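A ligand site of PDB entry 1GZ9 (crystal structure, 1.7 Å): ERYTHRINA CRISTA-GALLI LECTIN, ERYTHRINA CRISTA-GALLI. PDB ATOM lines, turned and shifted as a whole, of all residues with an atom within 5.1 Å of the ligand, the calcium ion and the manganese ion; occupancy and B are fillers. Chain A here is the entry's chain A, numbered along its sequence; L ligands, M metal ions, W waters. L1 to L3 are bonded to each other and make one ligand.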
ATOM      1  N   LEU A  86      18.504 -21.247 -14.083  1.00  0.00           N
ATOM      2  CA  LEU A  86      19.389 -20.289 -14.788  1.00  0.00           C
ATOM      3  C   LEU A  86      18.758 -18.896 -14.686  1.00  0.00           C
ATOM      4  O   LEU A  86      17.537 -18.752 -14.753  1.00  0.00           O
ATOM      5  CB  LEU A  86      19.489 -20.654 -16.263  1.00  0.00           C
ATOM      6  CG  LEU A  86      20.270 -21.941 -16.572  1.00  0.00           C
ATOM      7  CD1 LEU A  86      20.217 -22.187 -18.098  1.00  0.00           C
ATOM      8  CD2 LEU A  86      21.709 -21.844 -16.074  1.00  0.00           C
ATOM      9  N   ALA A  88      17.639 -14.987 -15.823  1.00  0.00           N
ATOM     10  CA  ALA A  88      17.072 -14.463 -17.091  1.00  0.00           C
ATOM     11  C   ALA A  88      16.428 -13.125 -16.744  1.00  0.00           C
ATOM     12  O   ALA A  88      16.187 -12.872 -15.560  1.00  0.00           O
ATOM     13  CB  ALA A  88      16.019 -15.422 -17.625  1.00  0.00           C
ATOM     14  N   ASP A  89      16.170 -12.237 -17.707  1.00  0.00           N
ATOM     15  CA  ASP A  89      16.462 -12.404 -19.138  1.00  0.00           C
ATOM     16  C   ASP A  89      17.452 -11.328 -19.674  1.00  0.00           C
ATOM     17  O   ASP A  89      18.144 -11.575 -20.670  1.00  0.00           O
ATOM     18  CB  ASP A  89      15.168 -12.317 -19.936  1.00  0.00           C
ATOM     19  CG  ASP A  89      14.554 -13.690 -20.244  1.00  0.00           C
ATOM     20  OD1 ASP A  89      15.104 -14.428 -21.102  1.00  0.00           O
ATOM     21  OD2 ASP A  89      13.512 -14.033 -19.619  1.00  0.00           O
ATOM     22  N   TYR A 106      10.166 -11.683 -21.066  1.00  0.00           N
ATOM     23  CA  TYR A 106      11.108 -12.785 -21.097  1.00  0.00           C
ATOM     24  C   TYR A 106      12.242 -12.463 -22.057  1.00  0.00           C
ATOM     25  O   TYR A 106      12.735 -11.328 -22.050  1.00  0.00           O
ATOM     26  CB  TYR A 106      10.396 -14.076 -21.512  1.00  0.00           C
ATOM     27  CG  TYR A 106       9.134 -14.252 -20.713  1.00  0.00           C
ATOM     28  CD1 TYR A 106       9.150 -14.115 -19.321  1.00  0.00           C
ATOM     29  CD2 TYR A 106       7.949 -14.628 -21.334  1.00  0.00           C
ATOM     30  CE1 TYR A 106       8.010 -14.368 -18.557  1.00  0.00           C
ATOM     31  CE2 TYR A 106       6.785 -14.887 -20.571  1.00  0.00           C
ATOM     32  CZ  TYR A 106       6.834 -14.760 -19.194  1.00  0.00           C
ATOM     33  OH  TYR A 106       5.693 -15.037 -18.444  1.00  0.00           O
ATOM     34  N   GLY A 107      12.611 -13.427 -22.896  1.00  0.00           N
ATOM     35  CA  GLY A 107      13.724 -13.233 -23.812  1.00  0.00           C
ATOM     36  C   GLY A 107      13.498 -12.147 -24.874  1.00  0.00           C
ATOM     37  O   GLY A 107      14.448 -11.769 -25.594  1.00  0.00           O
ATOM     38  N   TYR A 108      12.287 -11.625 -24.979  1.00  0.00           N
ATOM     39  CA  TYR A 108      12.012 -10.579 -25.963  1.00  0.00           C
ATOM     40  C   TYR A 108      12.296  -9.196 -25.392  1.00  0.00           C
ATOM     41  O   TYR A 108      12.179  -8.175 -26.102  1.00  0.00           O
ATOM     42  CB  TYR A 108      10.573 -10.676 -26.461  1.00  0.00           C
ATOM     43  CG  TYR A 108      10.289 -12.064 -27.009  1.00  0.00           C
ATOM     44  CD1 TYR A 108      10.772 -12.463 -28.249  1.00  0.00           C
ATOM     45  CD2 TYR A 108       9.588 -13.017 -26.232  1.00  0.00           C
ATOM     46  CE1 TYR A 108      10.576 -13.766 -28.726  1.00  0.00           C
ATOM     47  CE2 TYR A 108       9.389 -14.325 -26.701  1.00  0.00           C
ATOM     48  CZ  TYR A 108       9.891 -14.680 -27.946  1.00  0.00           C
ATOM     49  OH  TYR A 108       9.752 -15.984 -28.386  1.00  0.00           O
ATOM     50  N   GLU A 127      21.412  -4.837 -26.495  1.00  0.00           N
ATOM     51  CA  GLU A 127      21.034  -5.708 -25.376  1.00  0.00           C
ATOM     52  C   GLU A 127      22.199  -6.215 -24.554  1.00  0.00           C
ATOM     53  O   GLU A 127      23.322  -6.258 -25.047  1.00  0.00           O
ATOM     54  CB  GLU A 127      20.267  -6.900 -25.933  1.00  0.00           C
ATOM     55  CG  GLU A 127      21.107  -7.808 -26.852  1.00  0.00           C
ATOM     56  CD  GLU A 127      20.423  -9.125 -27.209  1.00  0.00           C
ATOM     57  OE1 GLU A 127      19.227  -9.130 -27.637  1.00  0.00           O
ATOM     58  OE2 GLU A 127      21.138 -10.131 -27.069  1.00  0.00           O
ATOM     59  N   ASP A 129      22.214  -9.396 -22.612  1.00  0.00           N
ATOM     60  CA  ASP A 129      21.353 -10.600 -22.513  1.00  0.00           C
ATOM     61  C   ASP A 129      21.945 -11.658 -21.628  1.00  0.00           C
ATOM     62  O   ASP A 129      23.089 -12.074 -21.836  1.00  0.00           O
ATOM     63  CB  ASP A 129      21.188 -11.105 -23.971  1.00  0.00           C
ATOM     64  CG  ASP A 129      20.176 -12.230 -24.127  1.00  0.00           C
ATOM     65  OD1 ASP A 129      19.733 -12.782 -23.121  1.00  0.00           O
ATOM     66  OD2 ASP A 129      19.859 -12.546 -25.297  1.00  0.00           O
ATOM     67  N   PHE A 131      20.269 -14.786 -20.773  1.00  0.00           N
ATOM     68  CA  PHE A 131      19.739 -16.161 -20.912  1.00  0.00           C
ATOM     69  C   PHE A 131      19.807 -16.558 -22.357  1.00  0.00           C
ATOM     70  O   PHE A 131      19.299 -15.825 -23.220  1.00  0.00           O
ATOM     71  CB  PHE A 131      18.277 -16.205 -20.444  1.00  0.00           C
ATOM     72  CG  PHE A 131      17.646 -17.596 -20.587  1.00  0.00           C
ATOM     73  CD1 PHE A 131      17.708 -18.511 -19.554  1.00  0.00           C
ATOM     74  CD2 PHE A 131      17.025 -17.956 -21.791  1.00  0.00           C
ATOM     75  CE1 PHE A 131      17.156 -19.810 -19.710  1.00  0.00           C
ATOM     76  CE2 PHE A 131      16.477 -19.250 -21.956  1.00  0.00           C
ATOM     77  CZ  PHE A 131      16.546 -20.173 -20.924  1.00  0.00           C
ATOM     78  N   SER A 132      20.350 -17.744 -22.630  1.00  0.00           N
ATOM     79  CA  SER A 132      20.509 -18.191 -24.038  1.00  0.00           C
ATOM     80  C   SER A 132      19.218 -18.837 -24.570  1.00  0.00           C
ATOM     81  O   SER A 132      18.917 -20.016 -24.274  1.00  0.00           O
ATOM     82  CB  SER A 132      21.650 -19.209 -24.155  1.00  0.00           C
ATOM     83  OG  SER A 132      21.943 -19.478 -25.519  1.00  0.00           O
ATOM     84  N   ASN A 133      18.466 -18.050 -25.317  1.00  0.00           N
ATOM     85  CA  ASN A 133      17.212 -18.517 -25.956  1.00  0.00           C
ATOM     86  C   ASN A 133      17.564 -19.310 -27.245  1.00  0.00           C
ATOM     87  O   ASN A 133      18.709 -19.319 -27.685  1.00  0.00           O
ATOM     88  CB  ASN A 133      16.367 -17.299 -26.344  1.00  0.00           C
ATOM     89  CG  ASN A 133      15.812 -16.591 -25.128  1.00  0.00           C
ATOM     90  OD1 ASN A 133      16.432 -15.673 -24.574  1.00  0.00           O
ATOM     91  ND2 ASN A 133      14.640 -17.051 -24.658  1.00  0.00           N
ATOM     92  N   PRO A 134      16.572 -19.929 -27.887  1.00  0.00           N
ATOM     93  CA  PRO A 134      16.831 -20.705 -29.110  1.00  0.00           C
ATOM     94  C   PRO A 134      17.482 -19.919 -30.265  1.00  0.00           C
ATOM     95  O   PRO A 134      18.089 -20.538 -31.168  1.00  0.00           O
ATOM     96  CB  PRO A 134      15.424 -21.225 -29.492  1.00  0.00           C
ATOM     97  CG  PRO A 134      14.751 -21.378 -28.131  1.00  0.00           C
ATOM     98  CD  PRO A 134      15.179 -20.098 -27.420  1.00  0.00           C
ATOM     99  N   TRP A 135      17.388 -18.583 -30.250  1.00  0.00           N
ATOM    100  CA  TRP A 135      17.942 -17.740 -31.295  1.00  0.00           C
ATOM    101  C   TRP A 135      19.255 -17.071 -30.863  1.00  0.00           C
ATOM    102  O   TRP A 135      19.836 -16.280 -31.644  1.00  0.00           O
ATOM    103  CB  TRP A 135      16.959 -16.603 -31.641  1.00  0.00           C
ATOM    104  CG  TRP A 135      16.589 -15.766 -30.384  1.00  0.00           C
ATOM    105  CD1 TRP A 135      17.341 -14.760 -29.799  1.00  0.00           C
ATOM    106  CD2 TRP A 135      15.416 -15.911 -29.578  1.00  0.00           C
ATOM    107  NE1 TRP A 135      16.700 -14.275 -28.667  1.00  0.00           N
ATOM    108  CE2 TRP A 135      15.514 -14.960 -28.518  1.00  0.00           C
ATOM    109  CE3 TRP A 135      14.283 -16.747 -29.643  1.00  0.00           C
ATOM    110  CZ2 TRP A 135      14.516 -14.838 -27.540  1.00  0.00           C
ATOM    111  CZ3 TRP A 135      13.303 -16.624 -28.670  1.00  0.00           C
ATOM    112  CH2 TRP A 135      13.426 -15.651 -27.624  1.00  0.00           C
ATOM    113  N   ASP A 136      19.693 -17.368 -29.640  1.00  0.00           N
ATOM    114  CA  ASP A 136      20.909 -16.748 -29.082  1.00  0.00           C
ATOM    115  C   ASP A 136      22.191 -17.534 -29.208  1.00  0.00           C
ATOM    116  O   ASP A 136      22.172 -18.734 -29.395  1.00  0.00           O
ATOM    117  CB  ASP A 136      20.767 -16.570 -27.543  1.00  0.00           C
ATOM    118  CG  ASP A 136      19.964 -15.331 -27.148  1.00  0.00           C
ATOM    119  OD1 ASP A 136      20.190 -14.276 -27.738  1.00  0.00           O
ATOM    120  OD2 ASP A 136      19.123 -15.434 -26.234  1.00  0.00           O
ATOM    121  N   PRO A 137      23.344 -16.848 -29.079  1.00  0.00           N
ATOM    122  CA  PRO A 137      24.625 -17.531 -29.127  1.00  0.00           C
ATOM    123  C   PRO A 137      24.619 -18.211 -27.768  1.00  0.00           C
ATOM    124  O   PRO A 137      23.862 -17.816 -26.868  1.00  0.00           O
ATOM    125  CB  PRO A 137      25.642 -16.393 -29.169  1.00  0.00           C
ATOM    126  CG  PRO A 137      24.901 -15.235 -28.548  1.00  0.00           C
ATOM    127  CD  PRO A 137      23.532 -15.384 -29.164  1.00  0.00           C
ATOM    128  N   HIS A 142      25.790 -11.778 -22.903  1.00  0.00           N
ATOM    129  CA  HIS A 142      26.406 -11.245 -24.111  1.00  0.00           C
ATOM    130  C   HIS A 142      25.807  -9.865 -24.438  1.00  0.00           C
ATOM    131  O   HIS A 142      24.682  -9.530 -24.059  1.00  0.00           O
ATOM    132  CB  HIS A 142      26.261 -12.203 -25.341  1.00  0.00           C
ATOM    133  CG  HIS A 142      24.852 -12.576 -25.682  1.00  0.00           C
ATOM    134  ND1 HIS A 142      24.293 -13.775 -25.278  1.00  0.00           N
ATOM    135  CD2 HIS A 142      23.901 -11.943 -26.391  1.00  0.00           C
ATOM    136  CE1 HIS A 142      23.052 -13.852 -25.715  1.00  0.00           C
ATOM    137  NE2 HIS A 142      22.780 -12.754 -26.402  1.00  0.00           N
ATOM    138  N   ILE A 150      15.050  -9.619 -32.358  1.00  0.00           N
ATOM    139  CA  ILE A 150      15.694 -10.027 -31.104  1.00  0.00           C
ATOM    140  C   ILE A 150      16.911 -10.940 -31.460  1.00  0.00           C
ATOM    141  O   ILE A 150      17.769 -11.232 -30.609  1.00  0.00           O
ATOM    142  CB  ILE A 150      14.701 -10.834 -30.207  1.00  0.00           C
ATOM    143  CG1 ILE A 150      15.302 -11.033 -28.800  1.00  0.00           C
ATOM    144  CG2 ILE A 150      14.403 -12.182 -30.825  1.00  0.00           C
ATOM    145  CD1 ILE A 150      15.511  -9.717 -28.043  1.00  0.00           C
ATOM    146  N   SER A 152      20.199 -11.066 -32.751  1.00  0.00           N
ATOM    147  CA  SER A 152      21.243 -10.072 -33.016  1.00  0.00           C
ATOM    148  C   SER A 152      22.040 -10.249 -34.293  1.00  0.00           C
ATOM    149  O   SER A 152      22.389 -11.384 -34.636  1.00  0.00           O
ATOM    150  CB  SER A 152      22.252 -10.075 -31.872  1.00  0.00           C
ATOM    151  OG  SER A 152      21.598  -9.866 -30.638  1.00  0.00           O
ATOM    152  N   THR A 155      27.060 -10.259 -31.729  1.00  0.00           N
ATOM    153  CA  THR A 155      27.099 -10.350 -30.266  1.00  0.00           C
ATOM    154  C   THR A 155      28.527 -10.430 -29.770  1.00  0.00           C
ATOM    155  O   THR A 155      29.459 -10.750 -30.517  1.00  0.00           O
ATOM    156  CB  THR A 155      26.317 -11.598 -29.719  1.00  0.00           C
ATOM    157  OG1 THR A 155      26.862 -12.792 -30.299  1.00  0.00           O
ATOM    158  CG2 THR A 155      24.838 -11.527 -30.108  1.00  0.00           C
ATOM    159  N   THR A 216      12.643 -10.263 -16.446  1.00  0.00           N
ATOM    160  CA  THR A 216      13.065 -11.477 -15.743  1.00  0.00           C
ATOM    161  C   THR A 216      12.301 -12.611 -16.390  1.00  0.00           C
ATOM    162  O   THR A 216      11.454 -12.371 -17.263  1.00  0.00           O
ATOM    163  CB  THR A 216      12.851 -11.436 -14.199  1.00  0.00           C
ATOM    164  OG1 THR A 216      11.515 -11.064 -13.892  1.00  0.00           O
ATOM    165  CG2 THR A 216      13.821 -10.425 -13.601  1.00  0.00           C
ATOM    166  N   GLY A 217      12.612 -13.837 -15.972  1.00  0.00           N
ATOM    167  CA  GLY A 217      12.109 -15.028 -16.645  1.00  0.00           C
ATOM    168  C   GLY A 217      10.738 -15.629 -16.496  1.00  0.00           C
ATOM    169  O   GLY A 217       9.957 -15.188 -15.678  1.00  0.00           O
ATOM    170  N   ALA A 218      10.501 -16.673 -17.302  1.00  0.00           N
ATOM    171  CA  ALA A 218       9.193 -17.314 -17.364  1.00  0.00           C
ATOM    172  C   ALA A 218       8.933 -18.438 -16.401  1.00  0.00           C
ATOM    173  O   ALA A 218       7.923 -19.125 -16.528  1.00  0.00           O
ATOM    174  CB  ALA A 218       8.904 -17.779 -18.807  1.00  0.00           C
ATOM    175  N   GLN A 219       9.829 -18.654 -15.445  1.00  0.00           N
ATOM    176  CA  GLN A 219       9.568 -19.679 -14.454  1.00  0.00           C
ATOM    177  C   GLN A 219      10.149 -19.187 -13.148  1.00  0.00           C
ATOM    178  O   GLN A 219      11.008 -18.290 -13.133  1.00  0.00           O
ATOM    179  CB  GLN A 219      10.174 -21.040 -14.842  1.00  0.00           C
ATOM    180  CG  GLN A 219      11.684 -21.084 -14.825  1.00  0.00           C
ATOM    181  CD  GLN A 219      12.224 -22.492 -15.109  1.00  0.00           C
ATOM    182  OE1 GLN A 219      12.752 -23.149 -14.208  1.00  0.00           O
ATOM    183  NE2 GLN A 219      12.102 -22.936 -16.346  1.00  0.00           N
ATOM    184  N   ALA A 222      13.889 -17.601 -12.138  1.00  0.00           N
ATOM    185  CA  ALA A 222      14.736 -17.439 -13.346  1.00  0.00           C
ATOM    186  C   ALA A 222      14.721 -15.909 -13.338  1.00  0.00           C
ATOM    187  O   ALA A 222      13.940 -15.279 -14.060  1.00  0.00           O
ATOM    188  CB  ALA A 222      14.010 -17.991 -14.601  1.00  0.00           C
HETATM  189  C1  LIG L   1       9.287 -22.966 -19.049  1.00  0.00           C
HETATM  190  C2  LIG L   1       9.705 -21.500 -19.336  1.00  0.00           C
HETATM  191  C3  LIG L   1      10.315 -21.388 -20.746  1.00  0.00           C
HETATM  192  C4  LIG L   1       9.360 -21.938 -21.821  1.00  0.00           C
HETATM  193  C5  LIG L   1      10.027 -22.047 -23.191  1.00  0.00           C
HETATM  194  C6  LIG L   1       8.298 -23.395 -20.147  1.00  0.00           C
HETATM  195  O1  LIG L   1       7.922 -24.714 -19.909  1.00  0.00           O
HETATM  196  O2  LIG L   1       8.684 -23.011 -17.757  1.00  0.00           O
HETATM  197  O3  LIG L   1      10.616 -21.088 -18.342  1.00  0.00           O
HETATM  198  O4  LIG L   1      10.548 -19.953 -21.118  1.00  0.00           O
HETATM  199  O5  LIG L   1       8.971 -23.303 -21.456  1.00  0.00           O
HETATM  200  O6  LIG L   1       9.025 -22.032 -24.228  1.00  0.00           O
HETATM  201  C1  LG2 L   2      11.909 -19.419 -21.016  1.00  0.00           C
HETATM  202  C2  LG2 L   2      11.866 -18.118 -21.726  1.00  0.00           C
HETATM  203  C3  LG2 L   2      13.364 -17.537 -21.564  1.00  0.00           C
HETATM  204  C4  LG2 L   2      13.685 -17.381 -20.065  1.00  0.00           C
HETATM  205  C5  LG2 L   2      13.567 -18.796 -19.438  1.00  0.00           C
HETATM  206  C6  LG2 L   2      13.822 -18.804 -17.971  1.00  0.00           C
HETATM  207  O1  LG2 L   2      11.585 -18.448 -23.093  1.00  0.00           O
HETATM  208  O2  LG2 L   2      13.411 -16.238 -22.223  1.00  0.00           O
HETATM  209  O3  LG2 L   2      12.759 -16.524 -19.393  1.00  0.00           O
HETATM  210  O4  LG2 L   2      12.228 -19.295 -19.633  1.00  0.00           O
HETATM  211  O5  LG2 L   2      13.806 -20.186 -17.573  1.00  0.00           O
HETATM  212  C1  LG3 L   3      11.237 -17.510 -24.094  1.00  0.00           C
HETATM  213  C2  LG3 L   3      11.372 -18.303 -25.417  1.00  0.00           C
HETATM  214  C3  LG3 L   3      10.269 -19.369 -25.727  1.00  0.00           C
HETATM  215  C4  LG3 L   3       8.843 -18.816 -25.386  1.00  0.00           C
HETATM  216  C5  LG3 L   3       8.828 -18.248 -23.936  1.00  0.00           C
HETATM  217  C6  LG3 L   3       7.415 -17.657 -23.534  1.00  0.00           C
HETATM  218  O1  LG3 L   3      12.751 -18.630 -25.706  1.00  0.00           O
HETATM  219  O2  LG3 L   3      10.339 -19.684 -27.115  1.00  0.00           O
HETATM  220  O3  LG3 L   3       8.504 -17.784 -26.296  1.00  0.00           O
HETATM  221  O4  LG3 L   3       9.848 -17.118 -23.775  1.00  0.00           O
HETATM  222 CA    CA M   1      18.216 -14.112 -24.468  1.00  0.00          CA
HETATM  223 MN    MN M   2      20.702 -12.272 -27.284  1.00  0.00          MN
HETATM  224  O   HOH W   1      17.042 -12.667 -25.996  1.00  0.00           O
HETATM  225  O   HOH W   2      13.340 -20.959 -24.334  1.00  0.00           O
HETATM  226  O   HOH W   3      18.588 -11.589 -28.001  1.00  0.00           O
HETATM  227  O   HOH W   4      10.475 -25.414 -23.880  1.00  0.00           O
HETATM  228  O   HOH W   5       6.235 -21.399 -23.810  1.00  0.00           O
HETATM  229  O   HOH W   6      21.473 -12.249 -29.352  1.00  0.00           O
HETATM  230  O   HOH W   7      15.784 -20.640 -16.004  1.00  0.00           O
HETATM  231  O   HOH W   8      17.070 -13.418 -22.510  1.00  0.00           O
HETATM  232  O   HOH W   9       6.721 -21.528 -15.918  1.00  0.00           O
HETATM  233  O   HOH W  10       6.007 -17.029 -26.607  1.00  0.00           O
HETATM  234  O   HOH W  11      14.008 -22.410 -19.435  1.00  0.00           O
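The backbone NH of Gly 217 lies within hydrogen-bond range of the backbone carbonyl oxygen of Ala 222 (2.7 Å). OD1 of Asp 89 is in hydrogen-bond range of N of Gly 107 (3.2 Å).
The side-chain amide nitrogen of Asn 133 sits at hydrogen-bond distance from an oxygen (O1) of LG3 L3, at 2.7 Å. O3 of LIG L1 is in hydrogen-bond range of NE2 of Gln 219 (3.1 Å). O2 of LG2 L2 sits at hydrogen-bond distance from N of Gly 107 (3.0 Å). An oxygen (O3) of LG3 L3 sits at hydrogen-bond distance from the side-chain hydroxyl of Tyr 108. N of Ala 218 is in hydrogen-bond range of O3 of LG2 L2, at 3.1 Å. An oxygen (O3) of LG2 L2 sits at hydrogen-bond distance from the side-chain carboxylate of Asp 89, 2.6 Å away.
Four residues have an atom within 4 Å of the manganese ion: Glu 127, Asp 129, Asp 136 and His 142. Along chain A the residues within 4 Å of the manganese ion span positions 127 to 142. The nearest printed residue that does not touch the manganese ion is Ser 152 (4.2 Å).
Within 4 Å of the calcium ion: Asp 129, Phe 131, Asn 133 and Asp 136.
Water W1 bridges O of Gly 107 (2.8 Å) and NE1 of Trp 135 (3.1 Å). Water W3 lies within hydrogen-bond range of OE1 of Glu 127 (2.6 Å), O of Ile 150 (2.8 Å) and NE1 of Trp 135 (3.4 Å). Water W7 lies within hydrogen-bond range of O5 of LG2 L2 (2.6 Å) and O of Leu 86 (2.9 Å). Water W9 lies within hydrogen-bond range of the backbone carbonyl oxygen (O) of Ala 218 (2.8 Å) and an oxygen (O2) of LIG L1 (3.1 Å).
The manganese ion is bound by the side-chain carboxylate of Asp 136 (2.1 Å), the side-chain carboxylate of Asp 129 (2.2 Å), the side-chain carboxylate of Glu 127 (2.2 Å), water W6 (2.2 Å), a ring nitrogen (NE2) of His 142 (2.3 Å) and water W3 (2.3 Å). The manganese ion has six donor atoms within binding distance.
Residues that only touch the ligand: Ala 88, Tyr 106, Pro 134, Trp 135, Gly 217 and Ala 222. Hydrophobic or aromatic side chains within 4 Å of the ligand: Ala 88, Tyr 106, Tyr 108, Phe 131, Pro 134, Trp 135, Ala 218 and Ala 222. 13 residues have an atom within 4 Å of the ligand: Ala 88, Asp 89, Tyr 106, Gly 107, Tyr 108, Phe 131, Asn 133, Pro 134, Trp 135, Gly 217, Ala 218, Gln 219 and Ala 222. The nearest printed residue that does not touch the ligand is Thr 216 (4.8 Å).
The calcium ion is bound by water W8 (2.4 Å), the side-chain amide oxygen (OD1) of Asn 133 (2.4 Å), the backbone carbonyl oxygen (O) of Phe 131 (2.4 Å), the side-chain carboxylate (OD2) of Asp 136 (2.4 Å), water W1 (2.4 Å), the side-chain carboxylate (OD2) of Asp 129 (2.4 Å) and the side-chain carboxylate (OD1) of Asp 129 (2.4 Å). The calcium ion has seven donor atoms within binding distance.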
